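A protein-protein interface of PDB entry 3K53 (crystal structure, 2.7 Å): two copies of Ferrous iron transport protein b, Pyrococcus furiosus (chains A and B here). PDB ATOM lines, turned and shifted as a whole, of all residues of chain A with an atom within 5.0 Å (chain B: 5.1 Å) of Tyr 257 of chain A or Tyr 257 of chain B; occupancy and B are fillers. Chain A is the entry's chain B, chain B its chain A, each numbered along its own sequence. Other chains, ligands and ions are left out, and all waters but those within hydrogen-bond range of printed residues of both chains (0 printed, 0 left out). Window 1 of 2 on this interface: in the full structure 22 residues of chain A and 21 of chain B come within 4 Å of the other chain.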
ATOM      1  N   MET A  95     -32.188 -12.067 -11.736  1.00  0.00           N
ATOM      2  CA  MET A  95     -30.937 -11.544 -12.282  1.00  0.00           C
ATOM      3  C   MET A  95     -30.908 -11.544 -13.807  1.00  0.00           C
ATOM      4  O   MET A  95     -30.711 -10.490 -14.422  1.00  0.00           O
ATOM      5  CB  MET A  95     -29.714 -12.301 -11.751  1.00  0.00           C
ATOM      6  CG  MET A  95     -28.400 -11.707 -12.301  1.00  0.00           C
ATOM      7  SD  MET A  95     -26.855 -12.084 -11.428  1.00  0.00           S
ATOM      8  CE  MET A  95     -26.815 -10.742 -10.235  1.00  0.00           C
ATOM      9  N   PHE A  99     -31.857  -8.165 -16.507  1.00  0.00           N
ATOM     10  CA  PHE A  99     -30.755  -7.755 -17.360  1.00  0.00           C
ATOM     11  C   PHE A  99     -31.347  -7.112 -18.617  1.00  0.00           C
ATOM     12  O   PHE A  99     -30.833  -6.117 -19.115  1.00  0.00           O
ATOM     13  CB  PHE A  99     -29.886  -8.956 -17.735  1.00  0.00           C
ATOM     14  CG  PHE A  99     -28.718  -8.613 -18.627  1.00  0.00           C
ATOM     15  CD1 PHE A  99     -27.454  -8.404 -18.091  1.00  0.00           C
ATOM     16  CD2 PHE A  99     -28.889  -8.483 -20.004  1.00  0.00           C
ATOM     17  CE1 PHE A  99     -26.375  -8.071 -18.914  1.00  0.00           C
ATOM     18  CE2 PHE A  99     -27.820  -8.152 -20.833  1.00  0.00           C
ATOM     19  CZ  PHE A  99     -26.562  -7.945 -20.289  1.00  0.00           C
ATOM     20  N   ALA A 253     -21.490  -5.797 -19.285  1.00  0.00           N
ATOM     21  CA  ALA A 253     -22.418  -6.757 -18.725  1.00  0.00           C
ATOM     22  C   ALA A 253     -22.030  -7.059 -17.278  1.00  0.00           C
ATOM     23  O   ALA A 253     -22.876  -7.071 -16.383  1.00  0.00           O
ATOM     24  CB  ALA A 253     -22.416  -8.026 -19.557  1.00  0.00           C
ATOM     25  N   SER A 254     -20.742  -7.278 -17.046  1.00  0.00           N
ATOM     26  CA  SER A 254     -20.268  -7.588 -15.705  1.00  0.00           C
ATOM     27  C   SER A 254     -20.692  -6.515 -14.722  1.00  0.00           C
ATOM     28  O   SER A 254     -20.999  -6.798 -13.572  1.00  0.00           O
ATOM     29  CB  SER A 254     -18.736  -7.736 -15.684  1.00  0.00           C
ATOM     30  OG  SER A 254     -18.062  -6.496 -15.868  1.00  0.00           O
ATOM     31  N   GLN A 255     -20.709  -5.273 -15.177  1.00  0.00           N
ATOM     32  CA  GLN A 255     -21.085  -4.188 -14.295  1.00  0.00           C
ATOM     33  C   GLN A 255     -22.602  -4.061 -14.138  1.00  0.00           C
ATOM     34  O   GLN A 255     -23.082  -3.515 -13.140  1.00  0.00           O
ATOM     35  CB  GLN A 255     -20.443  -2.898 -14.791  1.00  0.00           C
ATOM     36  CG  GLN A 255     -18.933  -2.935 -14.649  1.00  0.00           C
ATOM     37  CD  GLN A 255     -18.279  -1.639 -15.050  1.00  0.00           C
ATOM     38  OE1 GLN A 255     -18.689  -0.561 -14.610  1.00  0.00           O
ATOM     39  NE2 GLN A 255     -17.253  -1.728 -15.888  1.00  0.00           N
ATOM     40  N   LYS A 256     -23.348  -4.572 -15.119  1.00  0.00           N
ATOM     41  CA  LYS A 256     -24.807  -4.564 -15.051  1.00  0.00           C
ATOM     42  C   LYS A 256     -25.225  -5.604 -13.997  1.00  0.00           C
ATOM     43  O   LYS A 256     -26.087  -5.335 -13.156  1.00  0.00           O
ATOM     44  CB  LYS A 256     -25.423  -4.962 -16.394  1.00  0.00           C
ATOM     45  CG  LYS A 256     -25.780  -3.834 -17.337  1.00  0.00           C
ATOM     46  CD  LYS A 256     -26.547  -4.413 -18.532  1.00  0.00           C
ATOM     47  CE  LYS A 256     -27.106  -3.349 -19.473  1.00  0.00           C
ATOM     48  NZ  LYS A 256     -26.080  -2.795 -20.384  1.00  0.00           N
ATOM     49  N   TYR A 257     -24.605  -6.778 -14.058  1.00  0.00           N
ATOM     50  CA  TYR A 257     -24.914  -7.864 -13.138  1.00  0.00           C
ATOM     51  C   TYR A 257     -24.703  -7.456 -11.683  1.00  0.00           C
ATOM     52  O   TYR A 257     -25.512  -7.787 -10.817  1.00  0.00           O
ATOM     53  CB  TYR A 257     -24.070  -9.098 -13.464  1.00  0.00           C
ATOM     54  CG  TYR A 257     -24.538  -9.854 -14.688  1.00  0.00           C
ATOM     55  CD1 TYR A 257     -23.648 -10.211 -15.690  1.00  0.00           C
ATOM     56  CD2 TYR A 257     -25.873 -10.209 -14.839  1.00  0.00           C
ATOM     57  CE1 TYR A 257     -24.072 -10.901 -16.811  1.00  0.00           C
ATOM     58  CE2 TYR A 257     -26.305 -10.900 -15.955  1.00  0.00           C
ATOM     59  CZ  TYR A 257     -25.401 -11.243 -16.938  1.00  0.00           C
ATOM     60  OH  TYR A 257     -25.828 -11.930 -18.050  1.00  0.00           O
ATOM     61  N   GLU A 258     -23.615  -6.739 -11.417  1.00  0.00           N
ATOM     62  CA  GLU A 258     -23.310  -6.324 -10.059  1.00  0.00           C
ATOM     63  C   GLU A 258     -24.315  -5.274  -9.620  1.00  0.00           C
ATOM     64  O   GLU A 258     -24.728  -5.252  -8.459  1.00  0.00           O
ATOM     65  CB  GLU A 258     -21.887  -5.763  -9.966  1.00  0.00           C
ATOM     66  CG  GLU A 258     -21.598  -5.008  -8.669  1.00  0.00           C
ATOM     67  CD  GLU A 258     -21.746  -5.868  -7.428  1.00  0.00           C
ATOM     68  OE1 GLU A 258     -22.289  -6.991  -7.545  1.00  0.00           O
ATOM     69  OE2 GLU A 258     -21.326  -5.415  -6.335  1.00  0.00           O
ATOM     70  N   PHE A 259     -24.700  -4.408 -10.557  1.00  0.00           N
ATOM     71  CA  PHE A 259     -25.674  -3.352 -10.289  1.00  0.00           C
ATOM     72  C   PHE A 259     -26.957  -4.032  -9.826  1.00  0.00           C
ATOM     73  O   PHE A 259     -27.619  -3.596  -8.880  1.00  0.00           O
ATOM     74  CB  PHE A 259     -25.948  -2.550 -11.562  1.00  0.00           C
ATOM     75  CG  PHE A 259     -26.933  -1.427 -11.374  1.00  0.00           C
ATOM     76  CD1 PHE A 259     -26.652  -0.368 -10.511  1.00  0.00           C
ATOM     77  CD2 PHE A 259     -28.143  -1.423 -12.062  1.00  0.00           C
ATOM     78  CE1 PHE A 259     -27.562   0.677 -10.337  1.00  0.00           C
ATOM     79  CE2 PHE A 259     -29.057  -0.380 -11.892  1.00  0.00           C
ATOM     80  CZ  PHE A 259     -28.764   0.669 -11.030  1.00  0.00           C
ATOM     81  N   LEU A 260     -27.282  -5.122 -10.509  1.00  0.00           N
ATOM     82  CA  LEU A 260     -28.462  -5.899 -10.204  1.00  0.00           C
ATOM     83  C   LEU A 260     -28.319  -6.645  -8.875  1.00  0.00           C
ATOM     84  O   LEU A 260     -29.274  -6.721  -8.111  1.00  0.00           O
ATOM     85  CB  LEU A 260     -28.738  -6.862 -11.359  1.00  0.00           C
ATOM     86  CG  LEU A 260     -29.225  -6.190 -12.649  1.00  0.00           C
ATOM     87  CD1 LEU A 260     -29.358  -7.217 -13.761  1.00  0.00           C
ATOM     88  CD2 LEU A 260     -30.571  -5.524 -12.392  1.00  0.00           C
ATOM     89  N   GLU A 261     -27.134  -7.182  -8.594  1.00  0.00           N
ATOM     90  CA  GLU A 261     -26.917  -7.902  -7.339  1.00  0.00           C
ATOM     91  C   GLU A 261     -27.090  -6.961  -6.163  1.00  0.00           C
ATOM     92  O   GLU A 261     -27.296  -7.402  -5.033  1.00  0.00           O
ATOM     93  CB  GLU A 261     -25.510  -8.505  -7.258  1.00  0.00           C
ATOM     94  CG  GLU A 261     -25.244  -9.215  -5.927  1.00  0.00           C
ATOM     95  CD  GLU A 261     -23.769  -9.399  -5.628  1.00  0.00           C
ATOM     96  OE1 GLU A 261     -23.051  -8.382  -5.571  1.00  0.00           O
ATOM     97  OE2 GLU A 261     -23.325 -10.555  -5.441  1.00  0.00           O
ATOM     98  N   MET B  95     -25.903 -17.798 -13.672  1.00  0.00           N
ATOM     99  CA  MET B  95     -25.195 -16.562 -13.308  1.00  0.00           C
ATOM    100  C   MET B  95     -25.393 -16.236 -11.819  1.00  0.00           C
ATOM    101  O   MET B  95     -24.426 -16.217 -11.061  1.00  0.00           O
ATOM    102  CB  MET B  95     -25.692 -15.395 -14.158  1.00  0.00           C
ATOM    103  CG  MET B  95     -24.812 -14.155 -14.140  1.00  0.00           C
ATOM    104  SD  MET B  95     -23.633 -14.150 -15.501  1.00  0.00           S
ATOM    105  CE  MET B  95     -22.250 -14.702 -14.702  1.00  0.00           C
ATOM    106  N   PHE B  99     -22.170 -17.204  -8.610  1.00  0.00           N
ATOM    107  CA  PHE B  99     -21.406 -16.186  -7.906  1.00  0.00           C
ATOM    108  C   PHE B  99     -21.006 -16.812  -6.578  1.00  0.00           C
ATOM    109  O   PHE B  99     -19.834 -16.790  -6.196  1.00  0.00           O
ATOM    110  CB  PHE B  99     -22.253 -14.944  -7.644  1.00  0.00           C
ATOM    111  CG  PHE B  99     -21.481 -13.800  -7.050  1.00  0.00           C
ATOM    112  CD1 PHE B  99     -21.018 -12.766  -7.853  1.00  0.00           C
ATOM    113  CD2 PHE B  99     -21.196 -13.767  -5.689  1.00  0.00           C
ATOM    114  CE1 PHE B  99     -20.284 -11.717  -7.315  1.00  0.00           C
ATOM    115  CE2 PHE B  99     -20.461 -12.722  -5.142  1.00  0.00           C
ATOM    116  CZ  PHE B  99     -20.005 -11.696  -5.961  1.00  0.00           C
ATOM    117  N   ALA B 253     -16.404  -7.627  -7.277  1.00  0.00           N
ATOM    118  CA  ALA B 253     -17.556  -8.453  -7.599  1.00  0.00           C
ATOM    119  C   ALA B 253     -17.827  -8.309  -9.077  1.00  0.00           C
ATOM    120  O   ALA B 253     -18.104  -9.281  -9.774  1.00  0.00           O
ATOM    121  CB  ALA B 253     -18.758  -7.997  -6.814  1.00  0.00           C
ATOM    122  N   SER B 254     -17.747  -7.073  -9.548  1.00  0.00           N
ATOM    123  CA  SER B 254     -17.980  -6.776 -10.951  1.00  0.00           C
ATOM    124  C   SER B 254     -17.120  -7.676 -11.824  1.00  0.00           C
ATOM    125  O   SER B 254     -17.617  -8.308 -12.743  1.00  0.00           O
ATOM    126  CB  SER B 254     -17.656  -5.311 -11.233  1.00  0.00           C
ATOM    127  OG  SER B 254     -17.850  -5.021 -12.602  1.00  0.00           O
ATOM    128  N   GLN B 255     -15.826  -7.730 -11.522  1.00  0.00           N
ATOM    129  CA  GLN B 255     -14.886  -8.559 -12.273  1.00  0.00           C
ATOM    130  C   GLN B 255     -15.119 -10.048 -12.046  1.00  0.00           C
ATOM    131  O   GLN B 255     -14.725 -10.879 -12.868  1.00  0.00           O
ATOM    132  CB  GLN B 255     -13.453  -8.227 -11.885  1.00  0.00           C
ATOM    133  CG  GLN B 255     -12.985  -6.870 -12.342  1.00  0.00           C
ATOM    134  CD  GLN B 255     -11.502  -6.682 -12.112  1.00  0.00           C
ATOM    135  OE1 GLN B 255     -10.676  -7.406 -12.676  1.00  0.00           O
ATOM    136  NE2 GLN B 255     -11.154  -5.711 -11.279  1.00  0.00           N
ATOM    137  N   LYS B 256     -15.741 -10.384 -10.924  1.00  0.00           N
ATOM    138  CA  LYS B 256     -16.038 -11.777 -10.605  1.00  0.00           C
ATOM    139  C   LYS B 256     -17.096 -12.278 -11.610  1.00  0.00           C
ATOM    140  O   LYS B 256     -17.025 -13.415 -12.086  1.00  0.00           O
ATOM    141  CB  LYS B 256     -16.562 -11.868  -9.174  1.00  0.00           C
ATOM    142  CG  LYS B 256     -16.352 -13.196  -8.517  1.00  0.00           C
ATOM    143  CD  LYS B 256     -17.004 -13.212  -7.141  1.00  0.00           C
ATOM    144  CE  LYS B 256     -16.260 -12.348  -6.129  1.00  0.00           C
ATOM    145  NZ  LYS B 256     -14.947 -12.956  -5.778  1.00  0.00           N
ATOM    146  N   TYR B 257     -18.057 -11.414 -11.938  1.00  0.00           N
ATOM    147  CA  TYR B 257     -19.107 -11.750 -12.899  1.00  0.00           C
ATOM    148  C   TYR B 257     -18.502 -11.778 -14.286  1.00  0.00           C
ATOM    149  O   TYR B 257     -18.893 -12.572 -15.137  1.00  0.00           O
ATOM    150  CB  TYR B 257     -20.230 -10.710 -12.883  1.00  0.00           C
ATOM    151  CG  TYR B 257     -21.199 -10.852 -11.743  1.00  0.00           C
ATOM    152  CD1 TYR B 257     -21.248  -9.906 -10.722  1.00  0.00           C
ATOM    153  CD2 TYR B 257     -22.069 -11.934 -11.680  1.00  0.00           C
ATOM    154  CE1 TYR B 257     -22.141 -10.032  -9.663  1.00  0.00           C
ATOM    155  CE2 TYR B 257     -22.966 -12.070 -10.627  1.00  0.00           C
ATOM    156  CZ  TYR B 257     -22.994 -11.114  -9.625  1.00  0.00           C
ATOM    157  OH  TYR B 257     -23.879 -11.244  -8.585  1.00  0.00           O
ATOM    158  N   GLU B 258     -17.554 -10.876 -14.507  1.00  0.00           N
ATOM    159  CA  GLU B 258     -16.854 -10.766 -15.779  1.00  0.00           C
ATOM    160  C   GLU B 258     -16.204 -12.125 -15.995  1.00  0.00           C
ATOM    161  O   GLU B 258     -16.211 -12.661 -17.093  1.00  0.00           O
ATOM    162  CB  GLU B 258     -15.793  -9.672 -15.669  1.00  0.00           C
ATOM    163  CG  GLU B 258     -15.385  -9.014 -16.965  1.00  0.00           C
ATOM    164  CD  GLU B 258     -14.391  -7.881 -16.731  1.00  0.00           C
ATOM    165  OE1 GLU B 258     -14.702  -6.963 -15.935  1.00  0.00           O
ATOM    166  OE2 GLU B 258     -13.299  -7.908 -17.344  1.00  0.00           O
ATOM    167  N   PHE B 259     -15.663 -12.679 -14.915  1.00  0.00           N
ATOM    168  CA  PHE B 259     -15.017 -13.982 -14.936  1.00  0.00           C
ATOM    169  C   PHE B 259     -16.042 -15.065 -15.245  1.00  0.00           C
ATOM    170  O   PHE B 259     -15.732 -16.051 -15.908  1.00  0.00           O
ATOM    171  CB  PHE B 259     -14.395 -14.273 -13.570  1.00  0.00           C
ATOM    172  CG  PHE B 259     -13.482 -15.475 -13.557  1.00  0.00           C
ATOM    173  CD1 PHE B 259     -12.163 -15.371 -14.004  1.00  0.00           C
ATOM    174  CD2 PHE B 259     -13.932 -16.703 -13.092  1.00  0.00           C
ATOM    175  CE1 PHE B 259     -11.314 -16.467 -13.984  1.00  0.00           C
ATOM    176  CE2 PHE B 259     -13.089 -17.805 -13.070  1.00  0.00           C
ATOM    177  CZ  PHE B 259     -11.778 -17.685 -13.517  1.00  0.00           C
ATOM    178  N   LEU B 260     -17.261 -14.877 -14.749  1.00  0.00           N
ATOM    179  CA  LEU B 260     -18.335 -15.847 -14.943  1.00  0.00           C
ATOM    180  C   LEU B 260     -18.888 -15.922 -16.353  1.00  0.00           C
ATOM    181  O   LEU B 260     -19.167 -17.004 -16.845  1.00  0.00           O
ATOM    182  CB  LEU B 260     -19.485 -15.570 -13.974  1.00  0.00           C
ATOM    183  CG  LEU B 260     -19.546 -16.310 -12.639  1.00  0.00           C
ATOM    184  CD1 LEU B 260     -20.730 -15.795 -11.849  1.00  0.00           C
ATOM    185  CD2 LEU B 260     -19.666 -17.811 -12.868  1.00  0.00           C
ATOM    186  N   GLU B 261     -19.058 -14.777 -16.998  1.00  0.00           N
ATOM    187  CA  GLU B 261     -19.588 -14.759 -18.353  1.00  0.00           C
ATOM    188  C   GLU B 261     -18.699 -15.553 -19.297  1.00  0.00           C
ATOM    189  O   GLU B 261     -19.183 -16.344 -20.097  1.00  0.00           O
ATOM    190  CB  GLU B 261     -19.707 -13.327 -18.839  1.00  0.00           C
ATOM    191  CG  GLU B 261     -20.698 -12.509 -18.065  1.00  0.00           C
ATOM    192  CD  GLU B 261     -20.308 -11.052 -18.031  1.00  0.00           C
ATOM    193  OE1 GLU B 261     -19.927 -10.517 -19.096  1.00  0.00           O
ATOM    194  OE2 GLU B 261     -20.382 -10.442 -16.943  1.00  0.00           O
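The side-chain carboxylate (OE1) of Glu 258 of chain A lies close to the side-chain carboxylate (OE1) of Glu 261 of chain A (2.5 Å).
N of Ser 254 of chain A lies close to OE2 of Glu 261 of chain B (3.2 Å).
OE1 of Glu 258 of chain B is in hydrogen-bond range of OG of Ser 254 of chain A, 3.4 Å away.
OH of Tyr 257 of chain B sits at hydrogen-bond distance from OE2 of Glu 261 of chain A, at 3.3 Å.
Of the 11 printed residues of chain A, 7 touch a printed residue of chain B.
Printed residues of chain A that touch a printed residue of chain B: Met 95, Ala 253, Ser 254, Gln 255, Tyr 257, Glu 258 and Glu 261.
Of the 11 printed residues of chain B, 7 touch a printed residue of chain A.
Hydrophobic or aromatic side chains of chain B that line the printed part of chain A: Met 95, Phe 99, Ala 253 and Tyr 257.
Among the printed residues, 14 pairs touch across the chains.
Among the printed residues, no Asp or Glu carboxylate lies within 4 Å of a Lys or Arg side-chain nitrogen of the other chain.
Met 95 of chain A touches Tyr 257 of chain B, and with the chains exchanged Tyr 257 of chain A touches Met 95 of chain B.
Ser 254 of chain A touches Glu 261 of chain B, but with the chains exchanged Glu 261 of chain A does not touch Ser 254 of chain B (6.8 Å).
Glu 258 of chain A touches Ala 253 of chain B, but with the chains exchanged Ala 253 of chain A does not touch Glu 258 of chain B (6.5 Å).
Glu 261 of chain A touches Phe 99 of chain B, but with the chains exchanged Phe 99 of chain A does not touch Glu 261 of chain B (6.7 Å).
Of the 14 pairs that touch across the chains among the printed residues, 7 have their exchanged pair printed and touching as well.
Among the printed residues, merely in contact across the chains: Gln 255 of chain A with Ser 254 of chain B (3.1 Å), Ser 254 of chain A with Ser 254 of chain B (3.2 Å), Met 95 of chain A with Tyr 257 of chain B (3.4 Å), Tyr 257 of chain A with Glu 261 of chain B (3.5 Å), Tyr 257 of chain A with Met 95 of chain B (3.5 Å), Glu 261 of chain A with Phe 99 of chain B (3.5 Å), Ala 253 of chain A with Glu 261 of chain B (3.6 Å), Glu 258 of chain A with Ala 253 of chain B (3.7 Å), Glu 258 of chain A with Tyr 257 of chain B (3.7 Å), Tyr 257 of chain A with Tyr 257 of chain B (3.8 Å) and Met 95 of chain A with Met 95 of chain B (3.98 Å).
Phe 99 of chain A touches none of the printed residues of chain B.
Of the printed residues of chain B, Ala 253 of chain A touches Glu 261.
Of the printed residues of chain B, Tyr 257 of chain A touches Met 95, Tyr 257 and Glu 261.
Of the printed residues of chain A, Met 95 of chain B touches Met 95 and Tyr 257.
Of chain A, only Met 95, Tyr 257, Glu 258 and Glu 261 come within 4 Å of Tyr 257 of chain B.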
